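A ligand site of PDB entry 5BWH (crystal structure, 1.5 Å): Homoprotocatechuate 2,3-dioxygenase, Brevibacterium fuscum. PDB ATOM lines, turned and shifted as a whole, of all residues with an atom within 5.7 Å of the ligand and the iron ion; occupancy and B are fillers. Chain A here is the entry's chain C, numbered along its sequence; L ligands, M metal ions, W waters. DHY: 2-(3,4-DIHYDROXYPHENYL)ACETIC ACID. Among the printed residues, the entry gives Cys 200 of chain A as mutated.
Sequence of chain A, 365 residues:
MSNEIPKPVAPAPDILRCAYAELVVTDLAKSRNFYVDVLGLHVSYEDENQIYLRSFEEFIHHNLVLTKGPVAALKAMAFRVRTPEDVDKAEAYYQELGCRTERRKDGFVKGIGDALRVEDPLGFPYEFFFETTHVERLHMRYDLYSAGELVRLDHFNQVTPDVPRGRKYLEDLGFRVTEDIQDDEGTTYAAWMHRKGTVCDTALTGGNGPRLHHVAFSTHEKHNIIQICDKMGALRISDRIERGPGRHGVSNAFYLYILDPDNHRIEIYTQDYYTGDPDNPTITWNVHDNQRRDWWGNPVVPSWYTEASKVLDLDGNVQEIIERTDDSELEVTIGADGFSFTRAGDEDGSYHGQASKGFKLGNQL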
ATOM      1  N   HIS A 155      33.384  30.422  12.207  1.00  0.00           N
ATOM      2  CA  HIS A 155      32.600  31.652  12.070  1.00  0.00           C
ATOM      3  C   HIS A 155      32.242  32.281  13.395  1.00  0.00           C
ATOM      4  O   HIS A 155      32.416  31.669  14.459  1.00  0.00           O
ATOM      5  CB  HIS A 155      31.340  31.422  11.215  1.00  0.00           C
ATOM      6  CG  HIS A 155      30.339  30.504  11.809  1.00  0.00           C
ATOM      7  ND1 HIS A 155      30.253  29.156  11.493  1.00  0.00           N
ATOM      8  CD2 HIS A 155      29.303  30.743  12.653  1.00  0.00           C
ATOM      9  CE1 HIS A 155      29.220  28.612  12.113  1.00  0.00           C
ATOM     10  NE2 HIS A 155      28.632  29.550  12.822  1.00  0.00           N
ATOM     11  N   ASN A 157      28.761  34.573  15.084  1.00  0.00           N
ATOM     12  CA  ASN A 157      27.358  34.902  14.919  1.00  0.00           C
ATOM     13  C   ASN A 157      27.005  36.034  15.892  1.00  0.00           C
ATOM     14  O   ASN A 157      27.275  35.941  17.092  1.00  0.00           O
ATOM     15  CB  ASN A 157      26.478  33.676  15.117  1.00  0.00           C
ATOM     16  CG  ASN A 157      25.029  33.920  14.787  1.00  0.00           C
ATOM     17  OD1 ASN A 157      24.405  34.838  15.344  1.00  0.00           O
ATOM     18  ND2 ASN A 157      24.467  33.114  13.897  1.00  0.00           N
ATOM     19  N   ILE A 181      16.553  33.682   6.755  1.00  0.00           N
ATOM     20  CA  ILE A 181      15.250  33.270   7.254  1.00  0.00           C
ATOM     21  C   ILE A 181      14.330  34.505   7.221  1.00  0.00           C
ATOM     22  O   ILE A 181      14.679  35.533   7.790  1.00  0.00           O
ATOM     23  CB  ILE A 181      15.341  32.735   8.706  1.00  0.00           C
ATOM     24  CG1 ILE A 181      16.200  31.464   8.739  1.00  0.00           C
ATOM     25  CG2 ILE A 181      13.958  32.437   9.249  1.00  0.00           C
ATOM     26  CD1 ILE A 181      16.464  30.922  10.136  1.00  0.00           C
ATOM     27  N   TRP A 192      23.192  34.741   6.938  1.00  0.00           N
ATOM     28  CA  TRP A 192      24.523  34.149   7.004  1.00  0.00           C
ATOM     29  C   TRP A 192      25.303  34.681   5.812  1.00  0.00           C
ATOM     30  O   TRP A 192      24.772  34.726   4.709  1.00  0.00           O
ATOM     31  CB  TRP A 192      24.411  32.619   6.892  1.00  0.00           C
ATOM     32  CG  TRP A 192      23.925  31.962   8.183  1.00  0.00           C
ATOM     33  CD1 TRP A 192      24.697  31.302   9.095  1.00  0.00           C
ATOM     34  CD2 TRP A 192      22.584  31.887   8.681  1.00  0.00           C
ATOM     35  NE1 TRP A 192      23.934  30.861  10.132  1.00  0.00           N
ATOM     36  CE2 TRP A 192      22.623  31.190   9.895  1.00  0.00           C
ATOM     37  CE3 TRP A 192      21.345  32.349   8.206  1.00  0.00           C
ATOM     38  CZ2 TRP A 192      21.482  30.926  10.643  1.00  0.00           C
ATOM     39  CZ3 TRP A 192      20.202  32.094   8.951  1.00  0.00           C
ATOM     40  CH2 TRP A 192      20.272  31.403  10.164  1.00  0.00           C
ATOM     41  N   CYS A 200      29.297  30.586   6.224  1.00  0.00           N
ATOM     42  CA  CYS A 200      29.588  31.920   6.756  1.00  0.00           C
ATOM     43  C   CYS A 200      30.949  32.141   7.392  1.00  0.00           C
ATOM     44  O   CYS A 200      31.673  31.197   7.746  1.00  0.00           O
ATOM     45  CB  CYS A 200      28.469  32.384   7.693  1.00  0.00           C
ATOM     46  SG  CYS A 200      28.541  31.766   9.365  1.00  0.00           S
ATOM     47  N   HIS A 214      27.507  33.488  19.232  1.00  0.00           N
ATOM     48  CA  HIS A 214      28.476  32.391  19.424  1.00  0.00           C
ATOM     49  C   HIS A 214      29.710  32.539  18.571  1.00  0.00           C
ATOM     50  O   HIS A 214      29.752  33.335  17.609  1.00  0.00           O
ATOM     51  CB  HIS A 214      27.827  31.019  19.183  1.00  0.00           C
ATOM     52  CG  HIS A 214      27.276  30.818  17.818  1.00  0.00           C
ATOM     53  ND1 HIS A 214      25.966  31.054  17.524  1.00  0.00           N
ATOM     54  CD2 HIS A 214      27.815  30.308  16.694  1.00  0.00           C
ATOM     55  CE1 HIS A 214      25.713  30.737  16.276  1.00  0.00           C
ATOM     56  NE2 HIS A 214      26.822  30.284  15.741  1.00  0.00           N
ATOM     57  N   ALA A 216      32.053  29.693  16.437  1.00  0.00           N
ATOM     58  CA  ALA A 216      31.969  28.314  15.952  1.00  0.00           C
ATOM     59  C   ALA A 216      33.307  27.754  15.514  1.00  0.00           C
ATOM     60  O   ALA A 216      34.051  28.415  14.775  1.00  0.00           O
ATOM     61  CB  ALA A 216      30.992  28.211  14.792  1.00  0.00           C
ATOM     62  N   ARG A 243      22.072  23.050  23.371  1.00  0.00           N
ATOM     63  CA  ARG A 243      21.193  22.689  22.259  1.00  0.00           C
ATOM     64  C   ARG A 243      21.924  21.739  21.331  1.00  0.00           C
ATOM     65  O   ARG A 243      23.073  21.956  20.997  1.00  0.00           O
ATOM     66  CB  ARG A 243      20.777  23.966  21.499  1.00  0.00           C
ATOM     67  CG  ARG A 243      19.980  23.713  20.240  1.00  0.00           C
ATOM     68  CD  ARG A 243      19.391  24.957  19.591  1.00  0.00           C
ATOM     69  NE  ARG A 243      18.983  24.532  18.255  1.00  0.00           N
ATOM     70  CZ  ARG A 243      19.179  25.205  17.117  1.00  0.00           C
ATOM     71  NH1 ARG A 243      19.625  26.453  17.084  1.00  0.00           N
ATOM     72  NH2 ARG A 243      18.918  24.593  15.964  1.00  0.00           N
ATOM     73  N   HIS A 248      21.614  20.991  10.987  1.00  0.00           N
ATOM     74  CA  HIS A 248      21.038  22.295  10.662  1.00  0.00           C
ATOM     75  C   HIS A 248      20.243  22.164   9.374  1.00  0.00           C
ATOM     76  O   HIS A 248      20.661  21.447   8.447  1.00  0.00           O
ATOM     77  CB  HIS A 248      22.119  23.321  10.418  1.00  0.00           C
ATOM     78  CG  HIS A 248      22.752  23.913  11.642  1.00  0.00           C
ATOM     79  ND1 HIS A 248      22.015  24.497  12.655  1.00  0.00           N
ATOM     80  CD2 HIS A 248      24.044  24.174  11.905  1.00  0.00           C
ATOM     81  CE1 HIS A 248      22.849  25.023  13.534  1.00  0.00           C
ATOM     82  NE2 HIS A 248      24.095  24.837  13.102  1.00  0.00           N
ATOM     83  N   GLY A 249      19.150  22.913   9.267  1.00  0.00           N
ATOM     84  CA  GLY A 249      18.541  23.204   7.979  1.00  0.00           C
ATOM     85  C   GLY A 249      19.403  24.197   7.199  1.00  0.00           C
ATOM     86  O   GLY A 249      20.172  23.819   6.303  1.00  0.00           O
ATOM     87  N   VAL A 250      19.341  25.456   7.589  1.00  0.00           N
ATOM     88  CA  VAL A 250      20.323  26.454   7.156  1.00  0.00           C
ATOM     89  C   VAL A 250      21.744  25.910   7.357  1.00  0.00           C
ATOM     90  O   VAL A 250      22.101  25.458   8.439  1.00  0.00           O
ATOM     91  CB  VAL A 250      20.194  27.769   7.952  1.00  0.00           C
ATOM     92  CG1 VAL A 250      21.329  28.725   7.626  1.00  0.00           C
ATOM     93  CG2 VAL A 250      18.856  28.443   7.650  1.00  0.00           C
ATOM     94  N   SER A 251      22.520  25.936   6.287  1.00  0.00           N
ATOM     95  CA  SER A 251      23.932  25.483   6.248  1.00  0.00           C
ATOM     96  C   SER A 251      24.126  23.983   5.979  1.00  0.00           C
ATOM     97  O   SER A 251      25.210  23.590   5.514  1.00  0.00           O
ATOM     98  CB  SER A 251      24.751  25.886   7.482  1.00  0.00           C
ATOM     99  OG  SER A 251      24.636  24.909   8.500  1.00  0.00           O
ATOM    100  N   TYR A 255      25.801  19.969  14.098  1.00  0.00           N
ATOM    101  CA  TYR A 255      26.083  21.027  15.063  1.00  0.00           C
ATOM    102  C   TYR A 255      25.811  20.641  16.503  1.00  0.00           C
ATOM    103  O   TYR A 255      25.113  19.685  16.813  1.00  0.00           O
ATOM    104  CB  TYR A 255      25.241  22.275  14.747  1.00  0.00           C
ATOM    105  CG  TYR A 255      23.787  22.137  15.135  1.00  0.00           C
ATOM    106  CD1 TYR A 255      22.843  21.639  14.250  1.00  0.00           C
ATOM    107  CD2 TYR A 255      23.345  22.461  16.420  1.00  0.00           C
ATOM    108  CE1 TYR A 255      21.509  21.497  14.619  1.00  0.00           C
ATOM    109  CE2 TYR A 255      22.032  22.312  16.787  1.00  0.00           C
ATOM    110  CZ  TYR A 255      21.115  21.825  15.888  1.00  0.00           C
ATOM    111  OH  TYR A 255      19.793  21.688  16.263  1.00  0.00           O
ATOM    112  N   TYR A 257      25.653  23.186  20.389  1.00  0.00           N
ATOM    113  CA  TYR A 257      25.928  24.429  21.146  1.00  0.00           C
ATOM    114  C   TYR A 257      26.165  24.115  22.618  1.00  0.00           C
ATOM    115  O   TYR A 257      25.340  23.464  23.270  1.00  0.00           O
ATOM    116  CB  TYR A 257      24.756  25.409  21.046  1.00  0.00           C
ATOM    117  CG  TYR A 257      24.475  25.866  19.640  1.00  0.00           C
ATOM    118  CD1 TYR A 257      25.209  26.912  19.066  1.00  0.00           C
ATOM    119  CD2 TYR A 257      23.523  25.235  18.860  1.00  0.00           C
ATOM    120  CE1 TYR A 257      24.954  27.332  17.764  1.00  0.00           C
ATOM    121  CE2 TYR A 257      23.244  25.661  17.585  1.00  0.00           C
ATOM    122  CZ  TYR A 257      23.955  26.692  17.036  1.00  0.00           C
ATOM    123  OH  TYR A 257      23.627  27.047  15.753  1.00  0.00           O
ATOM    124  N   GLU A 267      29.698  27.059  19.333  1.00  0.00           N
ATOM    125  CA  GLU A 267      29.142  26.075  18.417  1.00  0.00           C
ATOM    126  C   GLU A 267      30.249  25.172  17.928  1.00  0.00           C
ATOM    127  O   GLU A 267      31.356  25.618  17.651  1.00  0.00           O
ATOM    128  CB  GLU A 267      28.480  26.745  17.226  1.00  0.00           C
ATOM    129  CG  GLU A 267      27.774  25.735  16.329  1.00  0.00           C
ATOM    130  CD  GLU A 267      27.131  26.367  15.118  1.00  0.00           C
ATOM    131  OE1 GLU A 267      27.417  27.552  14.826  1.00  0.00           O
ATOM    132  OE2 GLU A 267      26.337  25.658  14.484  1.00  0.00           O
ATOM    133  N   TYR A 269      30.703  22.404  14.792  1.00  0.00           N
ATOM    134  CA  TYR A 269      30.102  22.481  13.472  1.00  0.00           C
ATOM    135  C   TYR A 269      30.903  21.591  12.517  1.00  0.00           C
ATOM    136  O   TYR A 269      32.129  21.538  12.589  1.00  0.00           O
ATOM    137  CB  TYR A 269      30.215  23.958  13.043  1.00  0.00           C
ATOM    138  CG  TYR A 269      29.599  24.463  11.785  1.00  0.00           C
ATOM    139  CD1 TYR A 269      28.303  24.988  11.779  1.00  0.00           C
ATOM    140  CD2 TYR A 269      30.341  24.578  10.632  1.00  0.00           C
ATOM    141  CE1 TYR A 269      27.761  25.562  10.639  1.00  0.00           C
ATOM    142  CE2 TYR A 269      29.808  25.153   9.490  1.00  0.00           C
ATOM    143  CZ  TYR A 269      28.518  25.639   9.491  1.00  0.00           C
ATOM    144  OH  TYR A 269      28.035  26.222   8.342  1.00  0.00           O
ATOM    145  N   ARG A 292      13.960  24.419   9.537  1.00  0.00           N
ATOM    146  CA  ARG A 292      14.897  25.459   9.072  1.00  0.00           C
ATOM    147  C   ARG A 292      16.159  25.535   9.959  1.00  0.00           C
ATOM    148  O   ARG A 292      17.224  25.898   9.493  1.00  0.00           O
ATOM    149  CB  ARG A 292      14.197  26.827   9.002  1.00  0.00           C
ATOM    150  CG  ARG A 292      14.069  27.514  10.340  1.00  0.00           C
ATOM    151  CD  ARG A 292      13.076  28.669  10.390  1.00  0.00           C
ATOM    152  NE  ARG A 292      13.011  29.144  11.772  1.00  0.00           N
ATOM    153  CZ  ARG A 292      12.401  28.521  12.779  1.00  0.00           C
ATOM    154  NH1 ARG A 292      11.731  27.383  12.597  1.00  0.00           N
ATOM    155  NH2 ARG A 292      12.486  29.028  14.011  1.00  0.00           N
ATOM    156  N   ARG A 293      16.000  25.292  11.260  1.00  0.00           N
ATOM    157  CA  ARG A 293      17.094  25.431  12.196  1.00  0.00           C
ATOM    158  C   ARG A 293      17.605  24.038  12.526  1.00  0.00           C
ATOM    159  O   ARG A 293      18.696  23.684  12.096  1.00  0.00           O
ATOM    160  CB  ARG A 293      16.658  26.246  13.424  1.00  0.00           C
ATOM    161  CG  ARG A 293      16.643  27.742  13.125  1.00  0.00           C
ATOM    162  CD  ARG A 293      16.615  28.631  14.366  1.00  0.00           C
ATOM    163  NE  ARG A 293      16.653  30.057  13.984  1.00  0.00           N
ATOM    164  CZ  ARG A 293      17.755  30.767  13.723  1.00  0.00           C
ATOM    165  NH1 ARG A 293      18.965  30.222  13.752  1.00  0.00           N
ATOM    166  NH2 ARG A 293      17.650  32.051  13.419  1.00  0.00           N
ATOM    167  N   ASP A 294      16.791  23.247  13.212  1.00  0.00           N
ATOM    168  CA  ASP A 294      17.049  21.801  13.326  1.00  0.00           C
ATOM    169  C   ASP A 294      16.263  21.073  12.249  1.00  0.00           C
ATOM    170  O   ASP A 294      15.038  21.051  12.261  1.00  0.00           O
ATOM    171  CB  ASP A 294      16.709  21.264  14.712  1.00  0.00           C
ATOM    172  CG  ASP A 294      17.250  19.862  14.935  1.00  0.00           C
ATOM    173  OD1 ASP A 294      18.477  19.728  15.222  1.00  0.00           O
ATOM    174  OD2 ASP A 294      16.446  18.897  14.805  1.00  0.00           O
ATOM    175  N   VAL A 300      13.864  24.416  19.336  1.00  0.00           N
ATOM    176  CA  VAL A 300      14.945  25.359  19.702  1.00  0.00           C
ATOM    177  C   VAL A 300      14.634  25.892  21.087  1.00  0.00           C
ATOM    178  O   VAL A 300      13.624  26.540  21.286  1.00  0.00           O
ATOM    179  CB  VAL A 300      15.080  26.496  18.655  1.00  0.00           C
ATOM    180  CG1 VAL A 300      16.178  27.476  19.020  1.00  0.00           C
ATOM    181  CG2 VAL A 300      15.344  25.897  17.271  1.00  0.00           C
ATOM    182  N   TRP A 304      18.440  29.897  23.544  1.00  0.00           N
ATOM    183  CA  TRP A 304      19.163  30.094  22.285  1.00  0.00           C
ATOM    184  C   TRP A 304      18.765  31.411  21.628  1.00  0.00           C
ATOM    185  O   TRP A 304      19.586  32.100  21.038  1.00  0.00           O
ATOM    186  CB  TRP A 304      18.920  28.932  21.316  1.00  0.00           C
ATOM    187  CG  TRP A 304      19.990  28.826  20.280  1.00  0.00           C
ATOM    188  CD1 TRP A 304      21.158  28.132  20.372  1.00  0.00           C
ATOM    189  CD2 TRP A 304      20.032  29.486  19.016  1.00  0.00           C
ATOM    190  NE1 TRP A 304      21.906  28.297  19.251  1.00  0.00           N
ATOM    191  CE2 TRP A 304      21.233  29.114  18.392  1.00  0.00           C
ATOM    192  CE3 TRP A 304      19.150  30.351  18.341  1.00  0.00           C
ATOM    193  CZ2 TRP A 304      21.606  29.592  17.132  1.00  0.00           C
ATOM    194  CZ3 TRP A 304      19.514  30.831  17.117  1.00  0.00           C
ATOM    195  CH2 TRP A 304      20.742  30.438  16.507  1.00  0.00           C
HETATM  196  C1  DHY L   1      21.917  27.769  12.117  1.00  0.00           C
HETATM  197  C2  DHY L   1      22.585  28.358  13.217  1.00  0.00           C
HETATM  198  C3  DHY L   1      23.975  28.509  13.163  1.00  0.00           C
HETATM  199  C4  DHY L   1      24.713  28.036  12.046  1.00  0.00           C
HETATM  200  C5  DHY L   1      24.053  27.575  10.902  1.00  0.00           C
HETATM  201  C6  DHY L   1      22.658  27.356  10.957  1.00  0.00           C
HETATM  202  C7  DHY L   1      20.401  27.590  12.196  1.00  0.00           C
HETATM  203  C8  DHY L   1      20.018  26.966  13.557  1.00  0.00           C
HETATM  204  O1  DHY L   1      20.002  25.723  13.689  1.00  0.00           O
HETATM  205  O2  DHY L   1      19.749  27.729  14.466  1.00  0.00           O
HETATM  206  O3  DHY L   1      24.666  28.944  14.231  1.00  0.00           O
HETATM  207  O4  DHY L   1      26.070  28.259  12.069  1.00  0.00           O
HETATM  208 FE    FE M   1      26.672  29.122  13.833  1.00  0.00          FE
HETATM  209  O   HOH W   1      26.926  28.574   9.465  1.00  0.00           O
HETATM  210  O   HOH W   2      26.041  31.148  12.483  1.00  0.00           O
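NE1 of Trp 192 touches C5 of the ligand, 3.4 Å away.
Val 250 touches the ligand.
OG of Ser 251 touches C5 of the ligand, 3.6 Å away.
Tyr 269 touches the ligand.
CH2 of Trp 304 touches O2 of the ligand (3.5 Å).
Of the 21 residues printed, 12 come within 4 Å of the ligand.
Three residues have an atom within 4 Å of the iron ion: His 155, His 214 and Glu 267.
O1 of the ligand sits at hydrogen-bond distance from ND1 of His 248 (2.6 Å).
O3 of the ligand sits close to OH of Tyr 257.
The backbone carbonyl oxygen (O) of Arg 293 sits close to an oxygen (O1) of the ligand (2.9 Å).
The guanidinium group (NH1) of Arg 293 lies within salt-bridge range of an oxygen (O2) of the ligand (2.7 Å).
An oxygen (O1) of the ligand is in salt-bridge range of the guanidinium group of Arg 243 (2.8 Å).
The side-chain carboxylate of Glu 267 lies within hydrogen-bond range of a ring nitrogen (NE2) of His 248.
The side-chain carboxylate (OE2) of Glu 267 lies within hydrogen-bond range of the side-chain hydroxyl (OH) of Tyr 257.
O of His 155 lies within hydrogen-bond range of N of Ala 216, at 2.8 Å.
SG of Cys 200 sits close to ND1 of His 155, 3.8 Å away.
O of Arg 293 sits close to ND1 of His 248, 3.5 Å away.
The backbone NH (N) of Tyr 257 is in hydrogen-bond range of the backbone carbonyl oxygen (O) of Arg 243 (2.9 Å).
The backbone carbonyl oxygen (O) of Arg 293 lies within hydrogen-bond range of the backbone NH (N) of Gly 249 (3.0 Å).
The guanidinium group (NH2) of Arg 243 is in hydrogen-bond range of the side-chain hydroxyl (OH) of Tyr 255, at 3.0 Å.
The iron ion is bound by the side-chain carboxylate (OE1) of Glu 267, an oxygen (O3) of the ligand, an oxygen (O4) of the ligand, a ring nitrogen (NE2) of His 214, a ring nitrogen (NE2) of His 155 and water W2.
Water W2 lies within hydrogen-bond range of the side-chain amide nitrogen of Asn 157 (2.9 Å) and the indole nitrogen of Trp 192 (3.2 Å).
Water W1 bridges OH of Tyr 269 (2.8 Å) and SG of Cys 200 (3.6 Å).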
